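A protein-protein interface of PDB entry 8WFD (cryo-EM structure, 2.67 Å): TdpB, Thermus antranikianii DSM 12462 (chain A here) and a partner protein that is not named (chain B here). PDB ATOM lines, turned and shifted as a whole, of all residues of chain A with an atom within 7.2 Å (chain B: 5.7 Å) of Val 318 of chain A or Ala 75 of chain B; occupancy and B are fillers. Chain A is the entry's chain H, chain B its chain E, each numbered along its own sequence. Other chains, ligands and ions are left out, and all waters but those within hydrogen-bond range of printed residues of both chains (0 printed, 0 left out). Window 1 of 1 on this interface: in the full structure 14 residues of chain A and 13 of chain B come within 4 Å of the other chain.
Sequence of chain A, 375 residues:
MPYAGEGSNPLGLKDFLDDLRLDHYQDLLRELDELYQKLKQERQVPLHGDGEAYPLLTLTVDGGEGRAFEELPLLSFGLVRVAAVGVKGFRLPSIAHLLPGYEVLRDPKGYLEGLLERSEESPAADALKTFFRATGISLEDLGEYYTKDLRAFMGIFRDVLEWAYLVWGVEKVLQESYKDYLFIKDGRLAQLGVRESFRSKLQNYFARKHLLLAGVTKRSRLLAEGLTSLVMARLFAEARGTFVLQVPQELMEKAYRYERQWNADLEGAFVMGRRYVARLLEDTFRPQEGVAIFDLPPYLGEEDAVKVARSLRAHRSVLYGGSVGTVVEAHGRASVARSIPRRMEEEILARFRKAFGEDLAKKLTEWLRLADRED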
ATOM      1  N   LEU A 281       5.404   7.184  -3.210  1.00  0.00           N
ATOM      2  CA  LEU A 281       4.449   6.089  -3.151  1.00  0.00           C
ATOM      3  C   LEU A 281       3.346   6.434  -2.162  1.00  0.00           C
ATOM      4  O   LEU A 281       3.591   7.059  -1.127  1.00  0.00           O
ATOM      5  CB  LEU A 281       5.127   4.777  -2.737  1.00  0.00           C
ATOM      6  CG  LEU A 281       6.206   4.231  -3.674  1.00  0.00           C
ATOM      7  CD1 LEU A 281       6.880   3.021  -3.053  1.00  0.00           C
ATOM      8  CD2 LEU A 281       5.620   3.882  -5.029  1.00  0.00           C
ATOM      9  N   ASP A 283       0.969   3.829  -1.196  1.00  0.00           N
ATOM     10  CA  ASP A 283       0.817   2.623  -0.393  1.00  0.00           C
ATOM     11  C   ASP A 283       2.200   2.053  -0.116  1.00  0.00           C
ATOM     12  O   ASP A 283       2.994   1.875  -1.045  1.00  0.00           O
ATOM     13  CB  ASP A 283      -0.056   1.591  -1.109  1.00  0.00           C
ATOM     14  CG  ASP A 283      -1.531   1.774  -0.818  1.00  0.00           C
ATOM     15  OD1 ASP A 283      -1.869   2.211   0.302  1.00  0.00           O
ATOM     16  OD2 ASP A 283      -2.354   1.479  -1.709  1.00  0.00           O
ATOM     17  N   PHE A 285       2.986  -0.225   3.160  1.00  0.00           N
ATOM     18  CA  PHE A 285       3.122  -1.313   4.125  1.00  0.00           C
ATOM     19  C   PHE A 285       3.869  -0.878   5.382  1.00  0.00           C
ATOM     20  O   PHE A 285       3.938  -1.638   6.352  1.00  0.00           O
ATOM     21  CB  PHE A 285       3.855  -2.517   3.518  1.00  0.00           C
ATOM     22  CG  PHE A 285       3.088  -3.241   2.450  1.00  0.00           C
ATOM     23  CD1 PHE A 285       1.720  -3.418   2.554  1.00  0.00           C
ATOM     24  CD2 PHE A 285       3.745  -3.766   1.350  1.00  0.00           C
ATOM     25  CE1 PHE A 285       1.024  -4.090   1.572  1.00  0.00           C
ATOM     26  CE2 PHE A 285       3.052  -4.438   0.369  1.00  0.00           C
ATOM     27  CZ  PHE A 285       1.692  -4.602   0.481  1.00  0.00           C
ATOM     28  N   HIS A 315      11.223   8.766 -12.078  1.00  0.00           N
ATOM     29  CA  HIS A 315      12.233   7.719 -11.961  1.00  0.00           C
ATOM     30  C   HIS A 315      12.078   6.896 -10.685  1.00  0.00           C
ATOM     31  O   HIS A 315      13.036   6.254 -10.247  1.00  0.00           O
ATOM     32  CB  HIS A 315      13.634   8.322 -12.039  1.00  0.00           C
ATOM     33  CG  HIS A 315      13.978   8.869 -13.390  1.00  0.00           C
ATOM     34  ND1 HIS A 315      13.404  10.014 -13.898  1.00  0.00           N
ATOM     35  CD2 HIS A 315      14.830   8.422 -14.341  1.00  0.00           C
ATOM     36  CE1 HIS A 315      13.892  10.253 -15.101  1.00  0.00           C
ATOM     37  NE2 HIS A 315      14.760   9.301 -15.395  1.00  0.00           N
ATOM     38  N   ARG A 316      10.886   6.881 -10.092  1.00  0.00           N
ATOM     39  CA  ARG A 316      10.688   6.177  -8.831  1.00  0.00           C
ATOM     40  C   ARG A 316      10.835   4.670  -9.015  1.00  0.00           C
ATOM     41  O   ARG A 316      10.645   4.131 -10.108  1.00  0.00           O
ATOM     42  CB  ARG A 316       9.310   6.496  -8.252  1.00  0.00           C
ATOM     43  CG  ARG A 316       8.161   5.864  -9.014  1.00  0.00           C
ATOM     44  CD  ARG A 316       6.837   6.096  -8.311  1.00  0.00           C
ATOM     45  NE  ARG A 316       5.724   5.512  -9.049  1.00  0.00           N
ATOM     46  CZ  ARG A 316       4.484   5.423  -8.589  1.00  0.00           C
ATOM     47  NH1 ARG A 316       4.158   5.873  -7.389  1.00  0.00           N
ATOM     48  NH2 ARG A 316       3.547   4.867  -9.351  1.00  0.00           N
ATOM     49  N   SER A 317      11.178   3.989  -7.922  1.00  0.00           N
ATOM     50  CA  SER A 317      11.303   2.539  -7.905  1.00  0.00           C
ATOM     51  C   SER A 317      10.698   1.996  -6.618  1.00  0.00           C
ATOM     52  O   SER A 317      10.438   2.738  -5.667  1.00  0.00           O
ATOM     53  CB  SER A 317      12.765   2.094  -8.034  1.00  0.00           C
ATOM     54  OG  SER A 317      12.858   0.687  -8.171  1.00  0.00           O
ATOM     55  N   VAL A 318      10.473   0.683  -6.599  1.00  0.00           N
ATOM     56  CA  VAL A 318       9.906   0.006  -5.436  1.00  0.00           C
ATOM     57  C   VAL A 318      10.915  -0.997  -4.896  1.00  0.00           C
ATOM     58  O   VAL A 318      10.539  -2.034  -4.340  1.00  0.00           O
ATOM     59  CB  VAL A 318       8.580  -0.697  -5.783  1.00  0.00           C
ATOM     60  CG1 VAL A 318       7.546   0.309  -6.254  1.00  0.00           C
ATOM     61  CG2 VAL A 318       8.810  -1.773  -6.828  1.00  0.00           C
ATOM     62  N   LEU A 319      12.205  -0.699  -5.056  1.00  0.00           N
ATOM     63  CA  LEU A 319      13.239  -1.678  -4.737  1.00  0.00           C
ATOM     64  C   LEU A 319      13.541  -1.715  -3.243  1.00  0.00           C
ATOM     65  O   LEU A 319      13.378  -2.752  -2.591  1.00  0.00           O
ATOM     66  CB  LEU A 319      14.509  -1.372  -5.533  1.00  0.00           C
ATOM     67  CG  LEU A 319      14.570  -2.014  -6.917  1.00  0.00           C
ATOM     68  CD1 LEU A 319      15.960  -1.882  -7.514  1.00  0.00           C
ATOM     69  CD2 LEU A 319      14.146  -3.464  -6.837  1.00  0.00           C
ATOM     70  N   TYR A 320      13.989  -0.595  -2.685  1.00  0.00           N
ATOM     71  CA  TYR A 320      14.365  -0.504  -1.278  1.00  0.00           C
ATOM     72  C   TYR A 320      13.335   0.286  -0.478  1.00  0.00           C
ATOM     73  O   TYR A 320      13.676   1.026   0.447  1.00  0.00           O
ATOM     74  CB  TYR A 320      15.750   0.121  -1.130  1.00  0.00           C
ATOM     75  CG  TYR A 320      16.885  -0.782  -1.558  1.00  0.00           C
ATOM     76  CD1 TYR A 320      16.986  -1.232  -2.867  1.00  0.00           C
ATOM     77  CD2 TYR A 320      17.857  -1.180  -0.652  1.00  0.00           C
ATOM     78  CE1 TYR A 320      18.022  -2.056  -3.260  1.00  0.00           C
ATOM     79  CE2 TYR A 320      18.897  -2.002  -1.036  1.00  0.00           C
ATOM     80  CZ  TYR A 320      18.975  -2.437  -2.341  1.00  0.00           C
ATOM     81  OH  TYR A 320      20.010  -3.257  -2.727  1.00  0.00           O
ATOM     82  N   GLY A 321      12.061   0.132  -0.823  1.00  0.00           N
ATOM     83  CA  GLY A 321      11.018   0.905  -0.185  1.00  0.00           C
ATOM     84  C   GLY A 321      10.916   2.304  -0.754  1.00  0.00           C
ATOM     85  O   GLY A 321      11.102   3.291  -0.036  1.00  0.00           O
ATOM     86  N   GLY A 322      10.627   2.402  -2.049  1.00  0.00           N
ATOM     87  CA  GLY A 322      10.515   3.690  -2.702  1.00  0.00           C
ATOM     88  C   GLY A 322      11.834   4.409  -2.885  1.00  0.00           C
ATOM     89  O   GLY A 322      12.066   5.458  -2.276  1.00  0.00           O
ATOM     90  N   SER A 323      12.708   3.857  -3.722  1.00  0.00           N
ATOM     91  CA  SER A 323      13.982   4.482  -4.033  1.00  0.00           C
ATOM     92  C   SER A 323      13.830   5.405  -5.242  1.00  0.00           C
ATOM     93  O   SER A 323      12.727   5.653  -5.735  1.00  0.00           O
ATOM     94  CB  SER A 323      15.049   3.419  -4.284  1.00  0.00           C
ATOM     95  OG  SER A 323      15.072   2.467  -3.236  1.00  0.00           O
ATOM     96  N   VAL A 324      14.960   5.924  -5.732  1.00  0.00           N
ATOM     97  CA  VAL A 324      14.946   6.830  -6.878  1.00  0.00           C
ATOM     98  C   VAL A 324      15.307   6.127  -8.181  1.00  0.00           C
ATOM     99  O   VAL A 324      15.218   6.742  -9.253  1.00  0.00           O
ATOM    100  CB  VAL A 324      15.881   8.028  -6.607  1.00  0.00           C
ATOM    101  CG1 VAL A 324      16.258   8.745  -7.894  1.00  0.00           C
ATOM    102  CG2 VAL A 324      15.227   8.995  -5.635  1.00  0.00           C
ATOM    103  N   GLY A 325      15.694   4.855  -8.129  1.00  0.00           N
ATOM    104  CA  GLY A 325      15.942   4.091  -9.337  1.00  0.00           C
ATOM    105  C   GLY A 325      17.344   4.254  -9.884  1.00  0.00           C
ATOM    106  O   GLY A 325      18.166   3.336  -9.798  1.00  0.00           O
ATOM    107  N   TYR B  70       8.251  -9.613  -1.610  1.00  0.00           N
ATOM    108  CA  TYR B  70       8.030  -8.273  -1.082  1.00  0.00           C
ATOM    109  C   TYR B  70       8.088  -7.227  -2.186  1.00  0.00           C
ATOM    110  O   TYR B  70       7.257  -6.310  -2.223  1.00  0.00           O
ATOM    111  CB  TYR B  70       9.051  -7.965   0.011  1.00  0.00           C
ATOM    112  CG  TYR B  70       8.690  -6.759   0.846  1.00  0.00           C
ATOM    113  CD1 TYR B  70       7.735  -6.844   1.846  1.00  0.00           C
ATOM    114  CD2 TYR B  70       9.304  -5.535   0.630  1.00  0.00           C
ATOM    115  CE1 TYR B  70       7.402  -5.746   2.607  1.00  0.00           C
ATOM    116  CE2 TYR B  70       8.978  -4.432   1.386  1.00  0.00           C
ATOM    117  CZ  TYR B  70       8.027  -4.542   2.373  1.00  0.00           C
ATOM    118  OH  TYR B  70       7.699  -3.442   3.129  1.00  0.00           O
ATOM    119  N   THR B  71       9.055  -7.346  -3.099  1.00  0.00           N
ATOM    120  CA  THR B  71       9.153  -6.377  -4.186  1.00  0.00           C
ATOM    121  C   THR B  71       7.883  -6.360  -5.027  1.00  0.00           C
ATOM    122  O   THR B  71       7.327  -5.289  -5.311  1.00  0.00           O
ATOM    123  CB  THR B  71      10.368  -6.692  -5.058  1.00  0.00           C
ATOM    124  OG1 THR B  71      11.524  -6.851  -4.227  1.00  0.00           O
ATOM    125  CG2 THR B  71      10.618  -5.573  -6.050  1.00  0.00           C
ATOM    126  N   LEU B  72       7.397  -7.538  -5.423  1.00  0.00           N
ATOM    127  CA  LEU B  72       6.226  -7.612  -6.284  1.00  0.00           C
ATOM    128  C   LEU B  72       4.960  -7.183  -5.555  1.00  0.00           C
ATOM    129  O   LEU B  72       4.091  -6.557  -6.164  1.00  0.00           O
ATOM    130  CB  LEU B  72       6.078  -9.028  -6.839  1.00  0.00           C
ATOM    131  CG  LEU B  72       7.169  -9.475  -7.812  1.00  0.00           C
ATOM    132  CD1 LEU B  72       7.291 -10.987  -7.830  1.00  0.00           C
ATOM    133  CD2 LEU B  72       6.895  -8.946  -9.205  1.00  0.00           C
ATOM    134  N   ALA B  73       4.833  -7.497  -4.263  1.00  0.00           N
ATOM    135  CA  ALA B  73       3.668  -7.036  -3.515  1.00  0.00           C
ATOM    136  C   ALA B  73       3.660  -5.517  -3.380  1.00  0.00           C
ATOM    137  O   ALA B  73       2.608  -4.878  -3.525  1.00  0.00           O
ATOM    138  CB  ALA B  73       3.632  -7.701  -2.140  1.00  0.00           C
ATOM    139  N   LEU B  74       4.823  -4.923  -3.098  1.00  0.00           N
ATOM    140  CA  LEU B  74       4.903  -3.471  -2.994  1.00  0.00           C
ATOM    141  C   LEU B  74       4.589  -2.808  -4.328  1.00  0.00           C
ATOM    142  O   LEU B  74       3.911  -1.777  -4.367  1.00  0.00           O
ATOM    143  CB  LEU B  74       6.287  -3.060  -2.497  1.00  0.00           C
ATOM    144  CG  LEU B  74       6.452  -1.604  -2.065  1.00  0.00           C
ATOM    145  CD1 LEU B  74       5.339  -1.195  -1.115  1.00  0.00           C
ATOM    146  CD2 LEU B  74       7.808  -1.404  -1.421  1.00  0.00           C
ATOM    147  N   ALA B  75       5.075  -3.380  -5.430  1.00  0.00           N
ATOM    148  CA  ALA B  75       4.710  -2.850  -6.740  1.00  0.00           C
ATOM    149  C   ALA B  75       3.219  -3.008  -7.014  1.00  0.00           C
ATOM    150  O   ALA B  75       2.594  -2.104  -7.578  1.00  0.00           O
ATOM    151  CB  ALA B  75       5.526  -3.535  -7.832  1.00  0.00           C
ATOM    152  N   HIS B  76       2.636  -4.144  -6.626  1.00  0.00           N
ATOM    153  CA  HIS B  76       1.227  -4.398  -6.902  1.00  0.00           C
ATOM    154  C   HIS B  76       0.328  -3.409  -6.177  1.00  0.00           C
ATOM    155  O   HIS B  76      -0.619  -2.875  -6.766  1.00  0.00           O
ATOM    156  CB  HIS B  76       0.872  -5.829  -6.502  1.00  0.00           C
ATOM    157  CG  HIS B  76      -0.596  -6.121  -6.529  1.00  0.00           C
ATOM    158  ND1 HIS B  76      -1.328  -6.149  -7.696  1.00  0.00           N
ATOM    159  CD2 HIS B  76      -1.469  -6.397  -5.532  1.00  0.00           C
ATOM    160  CE1 HIS B  76      -2.588  -6.431  -7.416  1.00  0.00           C
ATOM    161  NE2 HIS B  76      -2.700  -6.585  -6.109  1.00  0.00           N
ATOM    162  N   ILE B  77       0.604  -3.147  -4.898  1.00  0.00           N
ATOM    163  CA  ILE B  77      -0.307  -2.296  -4.141  1.00  0.00           C
ATOM    164  C   ILE B  77      -0.304  -0.860  -4.650  1.00  0.00           C
ATOM    165  O   ILE B  77      -1.173  -0.070  -4.262  1.00  0.00           O
ATOM    166  CB  ILE B  77       0.017  -2.337  -2.637  1.00  0.00           C
ATOM    167  CG1 ILE B  77       1.179  -1.406  -2.303  1.00  0.00           C
ATOM    168  CG2 ILE B  77       0.323  -3.753  -2.206  1.00  0.00           C
ATOM    169  CD1 ILE B  77       1.511  -1.371  -0.833  1.00  0.00           C
ATOM    170  N   ASN B  78       0.643  -0.497  -5.513  1.00  0.00           N
ATOM    171  CA  ASN B  78       0.718   0.841  -6.083  1.00  0.00           C
ATOM    172  C   ASN B  78       0.307   0.882  -7.550  1.00  0.00           C
ATOM    173  O   ASN B  78       0.479   1.916  -8.202  1.00  0.00           O
ATOM    174  CB  ASN B  78       2.130   1.400  -5.923  1.00  0.00           C
ATOM    175  CG  ASN B  78       2.402   1.891  -4.521  1.00  0.00           C
ATOM    176  OD1 ASN B  78       2.039   3.008  -4.163  1.00  0.00           O
ATOM    177  ND2 ASN B  78       3.043   1.055  -3.714  1.00  0.00           N
ATOM    178  N   GLN B  79      -0.228  -0.215  -8.083  1.00  0.00           N
ATOM    179  CA  GLN B  79      -0.648  -0.283  -9.484  1.00  0.00           C
ATOM    180  C   GLN B  79       0.495   0.096 -10.419  1.00  0.00           C
ATOM    181  O   GLN B  79       0.298   0.745 -11.448  1.00  0.00           O
ATOM    182  CB  GLN B  79      -1.871   0.598  -9.736  1.00  0.00           C
ATOM    183  CG  GLN B  79      -3.109   0.180  -8.971  1.00  0.00           C
ATOM    184  CD  GLN B  79      -4.134   1.289  -8.886  1.00  0.00           C
ATOM    185  OE1 GLN B  79      -3.876   2.419  -9.300  1.00  0.00           O
ATOM    186  NE2 GLN B  79      -5.304   0.973  -8.346  1.00  0.00           N
ATOM    187  N   VAL B  80       1.705  -0.313 -10.056  1.00  0.00           N
ATOM    188  CA  VAL B  80       2.875  -0.063 -10.887  1.00  0.00           C
ATOM    189  C   VAL B  80       2.972  -1.154 -11.944  1.00  0.00           C
ATOM    190  O   VAL B  80       2.972  -2.348 -11.623  1.00  0.00           O
ATOM    191  CB  VAL B  80       4.149  -0.004 -10.030  1.00  0.00           C
ATOM    192  CG1 VAL B  80       5.381  -0.113 -10.909  1.00  0.00           C
ATOM    193  CG2 VAL B  80       4.180   1.279  -9.216  1.00  0.00           C
ATOM    194  N   LEU B  82       5.090  -3.192 -14.186  1.00  0.00           N
ATOM    195  CA  LEU B  82       6.502  -3.539 -14.293  1.00  0.00           C
ATOM    196  C   LEU B  82       6.857  -3.893 -15.730  1.00  0.00           C
ATOM    197  O   LEU B  82       7.559  -4.876 -15.988  1.00  0.00           O
ATOM    198  CB  LEU B  82       6.850  -4.697 -13.355  1.00  0.00           C
ATOM    199  CG  LEU B  82       6.814  -4.397 -11.856  1.00  0.00           C
ATOM    200  CD1 LEU B  82       7.202  -5.629 -11.058  1.00  0.00           C
ATOM    201  CD2 LEU B  82       7.719  -3.229 -11.514  1.00  0.00           C
ATOM    202  N   ASP B  86       9.036   0.578 -13.859  1.00  0.00           N
ATOM    203  CA  ASP B  86      10.064   0.226 -12.878  1.00  0.00           C
ATOM    204  C   ASP B  86      11.049  -0.755 -13.499  1.00  0.00           C
ATOM    205  O   ASP B  86      11.072  -1.946 -13.150  1.00  0.00           O
ATOM    206  CB  ASP B  86       9.434  -0.349 -11.610  1.00  0.00           C
ATOM    207  CG  ASP B  86      10.223  -0.011 -10.366  1.00  0.00           C
ATOM    208  OD1 ASP B  86      11.409   0.354 -10.493  1.00  0.00           O
ATOM    209  OD2 ASP B  86       9.654  -0.104  -9.260  1.00  0.00           O
ATOM    210  N   ALA B  89      13.232  -2.502 -10.791  1.00  0.00           N
ATOM    211  CA  ALA B  89      12.534  -3.536 -10.038  1.00  0.00           C
ATOM    212  C   ALA B  89      12.275  -4.769 -10.891  1.00  0.00           C
ATOM    213  O   ALA B  89      12.324  -5.893 -10.383  1.00  0.00           O
ATOM    214  CB  ALA B  89      11.220  -2.988  -9.482  1.00  0.00           C
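The side-chain amide nitrogen of Asn 78 of chain B sits at hydrogen-bond distance from the backbone carbonyl oxygen of Asp 283 of chain A, at 2.8 Å. The side-chain carboxylate of Asp 86 of chain B is in hydrogen-bond range of the side-chain hydroxyl of Ser 317 of chain A (2.8 Å). OD2 of Asp 86 of chain B is in hydrogen-bond range of N of Val 318 of chain A (2.9 Å). The side-chain carboxylate (OD2) of Asp 283 of chain A sits close to the backbone carbonyl oxygen (O) of Ile 77 of chain B (3.2 Å).
Among the printed residues, merely in contact across the chains: Leu 281 of chain A with Asn 78 of chain B (3.8 Å), Asp 283 of chain A with Leu 74 of chain B (3.9 Å), Phe 285 of chain A with Tyr 70 of chain B (3.97 Å), Phe 285 of chain A with Ala 73 of chain B (3.9 Å), Phe 285 of chain A with Leu 74 of chain B (3.9 Å), Phe 285 of chain A with Ile 77 of chain B (3.1 Å), Arg 316 of chain A with Val 80 of chain B (3.6 Å), Arg 316 of chain A with Asp 86 of chain B (3.9 Å), Val 318 of chain A with Thr 71 of chain B (3.9 Å), Val 318 of chain A with Ala 75 of chain B (3.9 Å), Val 318 of chain A with Ala 89 of chain B (3.8 Å) and Leu 319 of chain A with Ala 89 of chain B (3.6 Å).
The backbone carbonyl oxygen of Leu 74 of chain B sits at hydrogen-bond distance from the side-chain amide nitrogen of Asn 78 of chain B (3.0 Å). The backbone carbonyl oxygen of Ala 75 of chain B is in hydrogen-bond range of the backbone NH of Val 80 of chain B, 3.2 Å away. N of Ala 89 of chain B sits at hydrogen-bond distance from OD1 of Asp 86 of chain B (3.4 Å). The backbone NH (N) of Leu 319 of chain A lies close to the side-chain hydroxyl (OG) of Ser 317 of chain A (3.5 Å). O of Ser 323 of chain A lies within hydrogen-bond range of N of Ser 317 of chain A (3.2 Å).
Printed residues of chain B that touch a printed residue of chain A: Tyr 70, Thr 71, Ala 73, Leu 74, Ala 75, Ile 77, Asn 78, Val 80, Asp 86 and Ala 89.
Printed residues of chain B within 4 Å of Phe 285 of chain A: Tyr 70 (3.97 Å), Ala 73 (3.9 Å), Leu 74 (3.9 Å) and Ile 77 (3.1 Å). His 315 of chain A touches none of the printed residues of chain B. Val 318 of chain A touches four residues of chain B. Gly 321 of chain A touches none of the printed residues of chain B. Ala 75 of chain B touches just one residue of chain A: Val 318 (3.9 Å). Printed residues of chain A within 4 Å of Ile 77 of chain B: Asp 283 (3.2 Å) and Phe 285 (3.1 Å).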
